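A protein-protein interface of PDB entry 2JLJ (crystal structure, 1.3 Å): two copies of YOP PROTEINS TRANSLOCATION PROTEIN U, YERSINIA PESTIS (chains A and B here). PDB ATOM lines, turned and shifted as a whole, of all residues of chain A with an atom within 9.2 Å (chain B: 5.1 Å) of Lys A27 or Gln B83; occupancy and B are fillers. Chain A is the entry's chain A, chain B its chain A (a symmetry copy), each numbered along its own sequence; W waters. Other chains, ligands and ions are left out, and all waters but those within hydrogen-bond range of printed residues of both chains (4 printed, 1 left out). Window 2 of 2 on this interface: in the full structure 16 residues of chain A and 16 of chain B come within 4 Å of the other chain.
The side-chain amide nitrogen of Gln B83 sits at hydrogen-bond distance from the backbone carbonyl oxygen of Glu A23, at 3.2 Å.
NE2 of Gln B83 is in hydrogen-bond range of OG of Ser A26 (2.6 Å).
The guanidinium group (NE) of Arg A29 lies within salt-bridge range of the side-chain carboxylate (OD1) of Asp B79 (2.8 Å).
N of Glu A23 lies close to OG of Ser A21, 3.4 Å away.
The backbone carbonyl oxygen (O) of Glu A23 sits at hydrogen-bond distance from the side-chain hydroxyl (OG) of Ser A26 (2.7 Å).
Ser A26 touches Asp B79 (O to CB, 3.7 Å).
Ala B80 touches Ser A26.
Lys A27 touches Ala B80 (CA to CB, 3.7 Å).
CD of Lys A27 touches OE1 of Gln B83 (3.8 Å).
Gln A30 touches Ala B80.
Gln A30 touches Gln B81.
Of chain B, only Ala B80 (3.7 Å) and Gln B83 (3.8 Å) come within 4 Å of Lys A27.
No residue of chain A comes within 4 Å of Thr B84.
Printed residues of chain B within 4 Å of Glu A23: Gln B83 (3.2 Å).
Of the printed residues of chain A, Asp B79 touches Ser A26 and Arg A29.
Printed residues of chain A within 4 Å of Ala B80: Ser A26 (3.7 Å), Lys A27 (3.7 Å) and Gln A30 (3.3 Å).
Printed residues of chain B within 4 Å of Ser A26: Asp B79 (3.7 Å), Ala B80 (3.7 Å) and Gln B83 (2.6 Å).
Of the printed residues of chain B, Arg A29 touches Asp B79.
His A32 touches none of the printed residues of chain B.
The nearest printed residue of chain B that does not touch Lys A27 is Asp B79 (5.5 Å).
The nearest printed residue of chain B that does not touch Arg A29 is Ala B80 (6.1 Å).
Printed residues of chain A that touch a printed residue of chain B: Glu A23, Ser A26, Lys A27, Arg A29 and Gln A30.
Hydrophobic or aromatic side chains of chain B within 4 Å of the printed part of chain A: Ala B80.
Among the printed residues, Asp or Glu carboxylates within 4 Å of a Lys or Arg side-chain nitrogen of the other chain: Arg A29 with Asp B79 (2.8 Å).
No position is printed for both chains.
Of the 9 pairs that touch across the chains among the printed residues, none has its exchanged pair printed and touching as well.
Water W1 lies within hydrogen-bond range of OD2 of Asp B79 (2.5 Å), O of Arg A29 (3.3 Å) and N of Gln A30 (3.4 Å).
Water W2 lies within hydrogen-bond range of the side-chain carboxylate of Asp B79 (2.5 Å) and the guanidinium group of Arg A29 (3.3 Å).
Water W3 lies within hydrogen-bond range of the side-chain amide nitrogen of Gln B83 (2.9 Å), the backbone carbonyl oxygen of Asp B79 (2.9 Å) and the side-chain hydroxyl of Ser A26 (3.0 Å).
Water W4 lies within hydrogen-bond range of the side-chain amide nitrogen (NE2) of Gln A30 and the side-chain amide nitrogen (NE2) of Gln B81.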
ATOM      1  N   SER A  21      29.709  11.788 -26.756  1.00  0.00           N
ATOM      2  CA  SER A  21      29.324  11.221 -28.025  1.00  0.00           C
ATOM      3  C   SER A  21      28.286  10.097 -27.843  1.00  0.00           C
ATOM      4  O   SER A  21      28.134   9.579 -26.738  1.00  0.00           O
ATOM      5  CB  SER A  21      30.569  10.653 -28.671  1.00  0.00           C
ATOM      6  OG  SER A  21      31.036   9.563 -27.866  1.00  0.00           O
ATOM      7  N   PRO A  22      27.609   9.721 -28.939  1.00  0.00           N
ATOM      8  CA  PRO A  22      26.701   8.600 -28.810  1.00  0.00           C
ATOM      9  C   PRO A  22      27.469   7.352 -28.391  1.00  0.00           C
ATOM     10  O   PRO A  22      26.946   6.503 -27.663  1.00  0.00           O
ATOM     11  CB  PRO A  22      26.153   8.453 -30.225  1.00  0.00           C
ATOM     12  CG  PRO A  22      26.259   9.834 -30.774  1.00  0.00           C
ATOM     13  CD  PRO A  22      27.497  10.392 -30.256  1.00  0.00           C
ATOM     14  N   GLU A  23      28.720   7.253 -28.807  1.00  0.00           N
ATOM     15  CA  GLU A  23      29.522   6.079 -28.466  1.00  0.00           C
ATOM     16  C   GLU A  23      29.800   6.017 -26.976  1.00  0.00           C
ATOM     17  O   GLU A  23      29.642   4.933 -26.350  1.00  0.00           O
ATOM     18  CB  GLU A  23      30.810   6.097 -29.271  1.00  0.00           C
ATOM     19  CG  GLU A  23      30.630   5.807 -30.783  1.00  0.00           C
ATOM     20  CD  GLU A  23      30.077   6.975 -31.620  1.00  0.00           C
ATOM     21  OE1 GLU A  23      30.106   8.149 -31.148  1.00  0.00           O
ATOM     22  OE2 GLU A  23      29.632   6.687 -32.758  1.00  0.00           O
ATOM     23  N   ILE A  24      30.224   7.099 -26.346  1.00  0.00           N
ATOM     24  CA  ILE A  24      30.448   7.062 -24.925  1.00  0.00           C
ATOM     25  C   ILE A  24      29.179   6.866 -24.151  1.00  0.00           C
ATOM     26  O   ILE A  24      29.137   6.179 -23.133  1.00  0.00           O
ATOM     27  CB  ILE A  24      31.295   8.263 -24.392  1.00  0.00           C
ATOM     28  CG1 ILE A  24      31.990   7.872 -23.064  1.00  0.00           C
ATOM     29  CG2 ILE A  24      30.501   9.563 -24.330  1.00  0.00           C
ATOM     30  CD1 ILE A  24      32.915   8.941 -22.489  1.00  0.00           C
ATOM     31  N   LYS A  25      28.059   7.402 -24.656  1.00  0.00           N
ATOM     32  CA  LYS A  25      26.778   7.115 -24.007  1.00  0.00           C
ATOM     33  C   LYS A  25      26.461   5.639 -23.965  1.00  0.00           C
ATOM     34  O   LYS A  25      25.948   5.135 -22.976  1.00  0.00           O
ATOM     35  CB  LYS A  25      25.636   7.880 -24.662  1.00  0.00           C
ATOM     36  CG  LYS A  25      25.718   9.365 -24.509  1.00  0.00           C
ATOM     37  CD  LYS A  25      24.674   9.993 -25.408  1.00  0.00           C
ATOM     38  CE  LYS A  25      24.360  11.421 -25.033  1.00  0.00           C
ATOM     39  NZ  LYS A  25      23.354  11.958 -26.031  1.00  0.00           N
ATOM     40  N   SER A  26      26.735   4.961 -25.071  1.00  0.00           N
ATOM     41  CA  SER A  26      26.498   3.531 -25.116  1.00  0.00           C
ATOM     42  C   SER A  26      27.395   2.755 -24.165  1.00  0.00           C
ATOM     43  O   SER A  26      26.960   1.769 -23.571  1.00  0.00           O
ATOM     44  CB  SER A  26      26.633   2.956 -26.522  1.00  0.00           C
ATOM     45  OG  SER A  26      27.949   2.909 -27.016  1.00  0.00           O
ATOM     46  N   LYS A  27      28.645   3.211 -23.980  1.00  0.00           N
ATOM     47  CA  LYS A  27      29.545   2.596 -23.013  1.00  0.00           C
ATOM     48  C   LYS A  27      29.012   2.841 -21.615  1.00  0.00           C
ATOM     49  O   LYS A  27      29.034   1.941 -20.770  1.00  0.00           O
ATOM     50  CB  LYS A  27      30.974   3.153 -23.183  1.00  0.00           C
ATOM     51  CG  LYS A  27      31.671   2.746 -24.465  1.00  0.00           C
ATOM     52  CD  LYS A  27      32.981   3.393 -24.760  1.00  0.00           C
ATOM     53  CE  LYS A  27      34.077   2.819 -23.898  1.00  0.00           C
ATOM     54  NZ  LYS A  27      35.462   3.315 -24.289  1.00  0.00           N
ATOM     55  N   ARG A  28      28.555   4.062 -21.341  1.00  0.00           N
ATOM     56  CA  ARG A  28      27.994   4.340 -19.999  1.00  0.00           C
ATOM     57  C   ARG A  28      26.771   3.514 -19.717  1.00  0.00           C
ATOM     58  O   ARG A  28      26.594   2.989 -18.632  1.00  0.00           O
ATOM     59  CB  ARG A  28      27.664   5.823 -19.895  1.00  0.00           C
ATOM     60  CG  ARG A  28      28.876   6.705 -19.738  1.00  0.00           C
ATOM     61  CD  ARG A  28      28.384   8.171 -19.551  1.00  0.00           C
ATOM     62  NE  ARG A  28      27.747   8.456 -18.249  1.00  0.00           N
ATOM     63  CZ  ARG A  28      26.918   9.502 -18.060  1.00  0.00           C
ATOM     64  NH1 ARG A  28      26.656  10.322 -19.056  1.00  0.00           N
ATOM     65  NH2 ARG A  28      26.325   9.722 -16.897  1.00  0.00           N
ATOM     66  N   ARG A  29      25.888   3.369 -20.700  1.00  0.00           N
ATOM     67  CA  ARG A  29      24.708   2.529 -20.474  1.00  0.00           C
ATOM     68  C   ARG A  29      25.083   1.121 -20.148  1.00  0.00           C
ATOM     69  O   ARG A  29      24.622   0.557 -19.152  1.00  0.00           O
ATOM     70  CB  ARG A  29      23.807   2.535 -21.706  1.00  0.00           C
ATOM     71  CG  ARG A  29      23.001   3.804 -21.854  1.00  0.00           C
ATOM     72  CD  ARG A  29      21.940   3.706 -22.979  1.00  0.00           C
ATOM     73  NE  ARG A  29      22.471   3.370 -24.281  1.00  0.00           N
ATOM     74  CZ  ARG A  29      22.829   4.258 -25.215  1.00  0.00           C
ATOM     75  NH1 ARG A  29      22.703   5.522 -25.021  1.00  0.00           N
ATOM     76  NH2 ARG A  29      23.253   3.815 -26.373  1.00  0.00           N
ATOM     77  N   GLN A  30      25.983   0.514 -20.922  1.00  0.00           N
ATOM     78  CA  GLN A  30      26.339  -0.847 -20.697  1.00  0.00           C
ATOM     79  C   GLN A  30      27.051  -0.989 -19.351  1.00  0.00           C
ATOM     80  O   GLN A  30      26.799  -1.915 -18.589  1.00  0.00           O
ATOM     81  CB  GLN A  30      27.209  -1.378 -21.817  1.00  0.00           C
ATOM     82  CG  GLN A  30      27.441  -2.877 -21.654  1.00  0.00           C
ATOM     83  CD  GLN A  30      28.408  -3.502 -22.623  1.00  0.00           C
ATOM     84  OE1 GLN A  30      28.858  -2.886 -23.549  1.00  0.00           O
ATOM     85  NE2 GLN A  30      28.686  -4.784 -22.417  1.00  0.00           N
ATOM     86  N   PHE A  31      27.981  -0.076 -19.033  1.00  0.00           N
ATOM     87  CA  PHE A  31      28.677  -0.185 -17.792  1.00  0.00           C
ATOM     88  C   PHE A  31      27.756  -0.105 -16.581  1.00  0.00           C
ATOM     89  O   PHE A  31      27.883  -0.901 -15.657  1.00  0.00           O
ATOM     90  CB  PHE A  31      29.799   0.880 -17.726  1.00  0.00           C
ATOM     91  CG  PHE A  31      30.465   0.923 -16.406  1.00  0.00           C
ATOM     92  CD1 PHE A  31      31.411  -0.015 -16.070  1.00  0.00           C
ATOM     93  CD2 PHE A  31      30.125   1.912 -15.490  1.00  0.00           C
ATOM     94  CE1 PHE A  31      31.964  -0.008 -14.791  1.00  0.00           C
ATOM     95  CE2 PHE A  31      30.713   1.915 -14.217  1.00  0.00           C
ATOM     96  CZ  PHE A  31      31.650   1.001 -13.914  1.00  0.00           C
ATOM     97  N   HIS A  32      26.864   0.871 -16.558  1.00  0.00           N
ATOM     98  CA  HIS A  32      25.998   1.018 -15.394  1.00  0.00           C
ATOM     99  C   HIS A  32      24.974  -0.083 -15.255  1.00  0.00           C
ATOM    100  O   HIS A  32      24.627  -0.475 -14.139  1.00  0.00           O
ATOM    101  CB  HIS A  32      25.376   2.415 -15.416  1.00  0.00           C
ATOM    102  CG  HIS A  32      26.360   3.451 -15.000  1.00  0.00           C
ATOM    103  ND1 HIS A  32      26.775   3.600 -13.691  1.00  0.00           N
ATOM    104  CD2 HIS A  32      27.127   4.290 -15.735  1.00  0.00           C
ATOM    105  CE1 HIS A  32      27.721   4.514 -13.637  1.00  0.00           C
ATOM    106  NE2 HIS A  32      27.945   4.961 -14.854  1.00  0.00           N
ATOM    107  N   GLN A  33      24.617  -0.738 -16.363  1.00  0.00           N
ATOM    108  CA  GLN A  33      23.862  -1.984 -16.315  1.00  0.00           C
ATOM    109  C   GLN A  33      24.683  -3.089 -15.670  1.00  0.00           C
ATOM    110  O   GLN A  33      24.240  -3.799 -14.755  1.00  0.00           O
ATOM    111  CB  GLN A  33      23.474  -2.343 -17.753  1.00  0.00           C
ATOM    112  CG  GLN A  33      22.423  -3.420 -17.962  1.00  0.00           C
ATOM    113  CD  GLN A  33      21.057  -2.946 -17.533  1.00  0.00           C
ATOM    114  OE1 GLN A  33      20.350  -2.144 -18.227  1.00  0.00           O
ATOM    115  NE2 GLN A  33      20.673  -3.423 -16.362  1.00  0.00           N
ATOM    116  N   GLU A  34      25.935  -3.254 -16.070  1.00  0.00           N
ATOM    117  CA  GLU A  34      26.745  -4.371 -15.624  1.00  0.00           C
ATOM    118  C   GLU A  34      27.166  -4.213 -14.174  1.00  0.00           C
ATOM    119  O   GLU A  34      27.286  -5.203 -13.451  1.00  0.00           O
ATOM    120  CB  GLU A  34      27.996  -4.518 -16.504  1.00  0.00           C
ATOM    121  CG  GLU A  34      27.710  -5.056 -17.854  1.00  0.00           C
ATOM    122  CD  GLU A  34      27.292  -6.505 -17.829  1.00  0.00           C
ATOM    123  OE1 GLU A  34      27.877  -7.271 -17.067  1.00  0.00           O
ATOM    124  OE2 GLU A  34      26.342  -6.859 -18.574  1.00  0.00           O
ATOM    125  N   ILE A  35      27.386  -2.976 -13.703  1.00  0.00           N
ATOM    126  CA  ILE A  35      27.841  -2.761 -12.341  1.00  0.00           C
ATOM    127  C   ILE A  35      26.708  -2.916 -11.332  1.00  0.00           C
ATOM    128  O   ILE A  35      26.957  -3.095 -10.146  1.00  0.00           O
ATOM    129  CB  ILE A  35      28.573  -1.398 -12.204  1.00  0.00           C
ATOM    130  CG1 ILE A  35      29.463  -1.385 -10.973  1.00  0.00           C
ATOM    131  CG2 ILE A  35      27.607  -0.257 -12.143  1.00  0.00           C
ATOM    132  CD1 ILE A  35      30.708  -2.078 -11.166  1.00  0.00           C
ATOM    133  N   LEU A 111      20.007   5.641 -18.711  1.00  0.00           N
ATOM    134  CA  LEU A 111      21.047   4.912 -17.942  1.00  0.00           C
ATOM    135  C   LEU A 111      20.422   4.390 -16.666  1.00  0.00           C
ATOM    136  O   LEU A 111      19.792   5.203 -15.929  1.00  0.00           O
ATOM    137  CB  LEU A 111      22.179   5.896 -17.558  1.00  0.00           C
ATOM    138  CG  LEU A 111      23.238   6.219 -18.615  1.00  0.00           C
ATOM    139  CD1 LEU A 111      22.616   6.888 -19.803  1.00  0.00           C
ATOM    140  CD2 LEU A 111      24.335   7.078 -17.899  1.00  0.00           C
ATOM    141  N   ASP B  79      24.227  -1.633 -27.425  1.00  0.00           N
ATOM    142  CA  ASP B  79      25.005  -0.606 -26.775  1.00  0.00           C
ATOM    143  C   ASP B  79      26.459  -0.753 -27.175  1.00  0.00           C
ATOM    144  O   ASP B  79      26.785  -0.795 -28.364  1.00  0.00           O
ATOM    145  CB  ASP B  79      24.728  -0.580 -25.275  1.00  0.00           C
ATOM    146  CG  ASP B  79      23.381   0.057 -24.969  1.00  0.00           C
ATOM    147  OD1 ASP B  79      23.020   0.984 -25.714  1.00  0.00           O
ATOM    148  OD2 ASP B  79      22.736  -0.339 -23.982  1.00  0.00           O
ATOM    149  N   ALA B  80      27.403  -0.707 -26.234  1.00  0.00           N
ATOM    150  CA  ALA B  80      28.821  -0.649 -26.590  1.00  0.00           C
ATOM    151  C   ALA B  80      29.326  -1.900 -27.251  1.00  0.00           C
ATOM    152  O   ALA B  80      30.353  -1.863 -27.920  1.00  0.00           O
ATOM    153  CB  ALA B  80      29.671  -0.289 -25.389  1.00  0.00           C
ATOM    154  N   GLN B  81      28.594  -2.991 -27.119  1.00  0.00           N
ATOM    155  CA  GLN B  81      28.965  -4.165 -27.830  1.00  0.00           C
ATOM    156  C   GLN B  81      28.929  -3.946 -29.346  1.00  0.00           C
ATOM    157  O   GLN B  81      29.659  -4.649 -30.081  1.00  0.00           O
ATOM    158  CB  GLN B  81      27.997  -5.319 -27.502  1.00  0.00           C
ATOM    159  CG  GLN B  81      27.966  -5.753 -26.084  1.00  0.00           C
ATOM    160  CD  GLN B  81      26.917  -6.815 -25.837  1.00  0.00           C
ATOM    161  OE1 GLN B  81      25.779  -6.758 -26.336  1.00  0.00           O
ATOM    162  NE2 GLN B  81      27.301  -7.817 -25.087  1.00  0.00           N
ATOM    163  N   VAL B  82      28.098  -3.022 -29.825  1.00  0.00           N
ATOM    164  CA  VAL B  82      28.015  -2.722 -31.255  1.00  0.00           C
ATOM    165  C   VAL B  82      29.365  -2.175 -31.747  1.00  0.00           C
ATOM    166  O   VAL B  82      29.797  -2.463 -32.857  1.00  0.00           O
ATOM    167  CB  VAL B  82      26.855  -1.742 -31.523  1.00  0.00           C
ATOM    168  CG1 VAL B  82      26.795  -1.365 -33.018  1.00  0.00           C
ATOM    169  CG2 VAL B  82      25.551  -2.339 -31.099  1.00  0.00           C
ATOM    170  N   GLN B  83      30.039  -1.409 -30.912  1.00  0.00           N
ATOM    171  CA  GLN B  83      31.387  -0.937 -31.253  1.00  0.00           C
ATOM    172  C   GLN B  83      32.326  -2.095 -31.512  1.00  0.00           C
ATOM    173  O   GLN B  83      33.099  -2.091 -32.489  1.00  0.00           O
ATOM    174  CB  GLN B  83      31.947  -0.070 -30.124  1.00  0.00           C
ATOM    175  CG  GLN B  83      31.177   1.213 -30.013  1.00  0.00           C
ATOM    176  CD  GLN B  83      31.409   1.963 -28.746  1.00  0.00           C
ATOM    177  OE1 GLN B  83      32.570   2.252 -28.380  1.00  0.00           O
ATOM    178  NE2 GLN B  83      30.290   2.357 -28.080  1.00  0.00           N
ATOM    179  N   THR B  84      32.298  -3.077 -30.611  1.00  0.00           N
ATOM    180  CA  THR B  84      33.161  -4.233 -30.761  1.00  0.00           C
ATOM    181  C   THR B  84      32.752  -5.046 -31.994  1.00  0.00           C
ATOM    182  O   THR B  84      33.623  -5.511 -32.741  1.00  0.00           O
ATOM    183  CB  THR B  84      33.121  -5.101 -29.519  1.00  0.00           C
ATOM    184  OG1 THR B  84      33.301  -4.253 -28.345  1.00  0.00           O
ATOM    185  CG2 THR B  84      34.222  -6.176 -29.618  1.00  0.00           C
ATOM    186  N   VAL B  85      31.458  -5.201 -32.241  1.00  0.00           N
ATOM    187  CA  VAL B  85      31.034  -5.891 -33.453  1.00  0.00           C
ATOM    188  C   VAL B  85      31.600  -5.192 -34.694  1.00  0.00           C
ATOM    189  O   VAL B  85      32.046  -5.870 -35.622  1.00  0.00           O
ATOM    190  CB  VAL B  85      29.487  -5.956 -33.510  1.00  0.00           C
ATOM    191  CG1 VAL B  85      28.999  -6.366 -34.917  1.00  0.00           C
ATOM    192  CG2 VAL B  85      28.976  -6.904 -32.487  1.00  0.00           C
ATOM    193  N   ARG B  86      31.521  -3.869 -34.738  1.00  0.00           N
ATOM    194  CA  ARG B  86      32.075  -3.095 -35.871  1.00  0.00           C
ATOM    195  C   ARG B  86      33.576  -3.333 -36.036  1.00  0.00           C
ATOM    196  O   ARG B  86      34.013  -3.561 -37.162  1.00  0.00           O
ATOM    197  CB  ARG B  86      31.788  -1.606 -35.706  1.00  0.00           C
ATOM    198  CG  ARG B  86      30.338  -1.213 -35.751  1.00  0.00           C
ATOM    199  CD  ARG B  86      30.172   0.297 -35.531  1.00  0.00           C
ATOM    200  NE  ARG B  86      28.776   0.674 -35.493  1.00  0.00           N
ATOM    201  CZ  ARG B  86      28.022   0.811 -36.579  1.00  0.00           C
ATOM    202  NH1 ARG B  86      28.543   0.634 -37.799  1.00  0.00           N
ATOM    203  NH2 ARG B  86      26.739   1.102 -36.443  1.00  0.00           N
ATOM    204  N   LYS B  87      34.307  -3.357 -34.924  1.00  0.00           N
ATOM    205  CA  LYS B  87      35.765  -3.623 -34.948  1.00  0.00           C
ATOM    206  C   LYS B  87      36.037  -5.020 -35.521  1.00  0.00           C
ATOM    207  O   LYS B  87      36.835  -5.206 -36.452  1.00  0.00           O
ATOM    208  CB  LYS B  87      36.355  -3.490 -33.544  1.00  0.00           C
ATOM    209  CG  LYS B  87      37.843  -3.803 -33.458  1.00  0.00           C
ATOM    210  CD  LYS B  87      38.387  -3.611 -32.025  1.00  0.00           C
ATOM    211  CE  LYS B  87      37.937  -4.686 -31.025  1.00  0.00           C
ATOM    212  NZ  LYS B  87      38.465  -4.465 -29.619  1.00  0.00           N
HETATM  213  O   HOH W   1      23.001  -1.086 -21.576  1.00  0.00           O
HETATM  214  O   HOH W   2      20.729   1.716 -26.556  1.00  0.00           O
HETATM  215  O   HOH W   3      28.031   1.509 -29.660  1.00  0.00           O
HETATM  216  O   HOH W   4      29.952  -7.500 -23.294  1.00  0.00           O
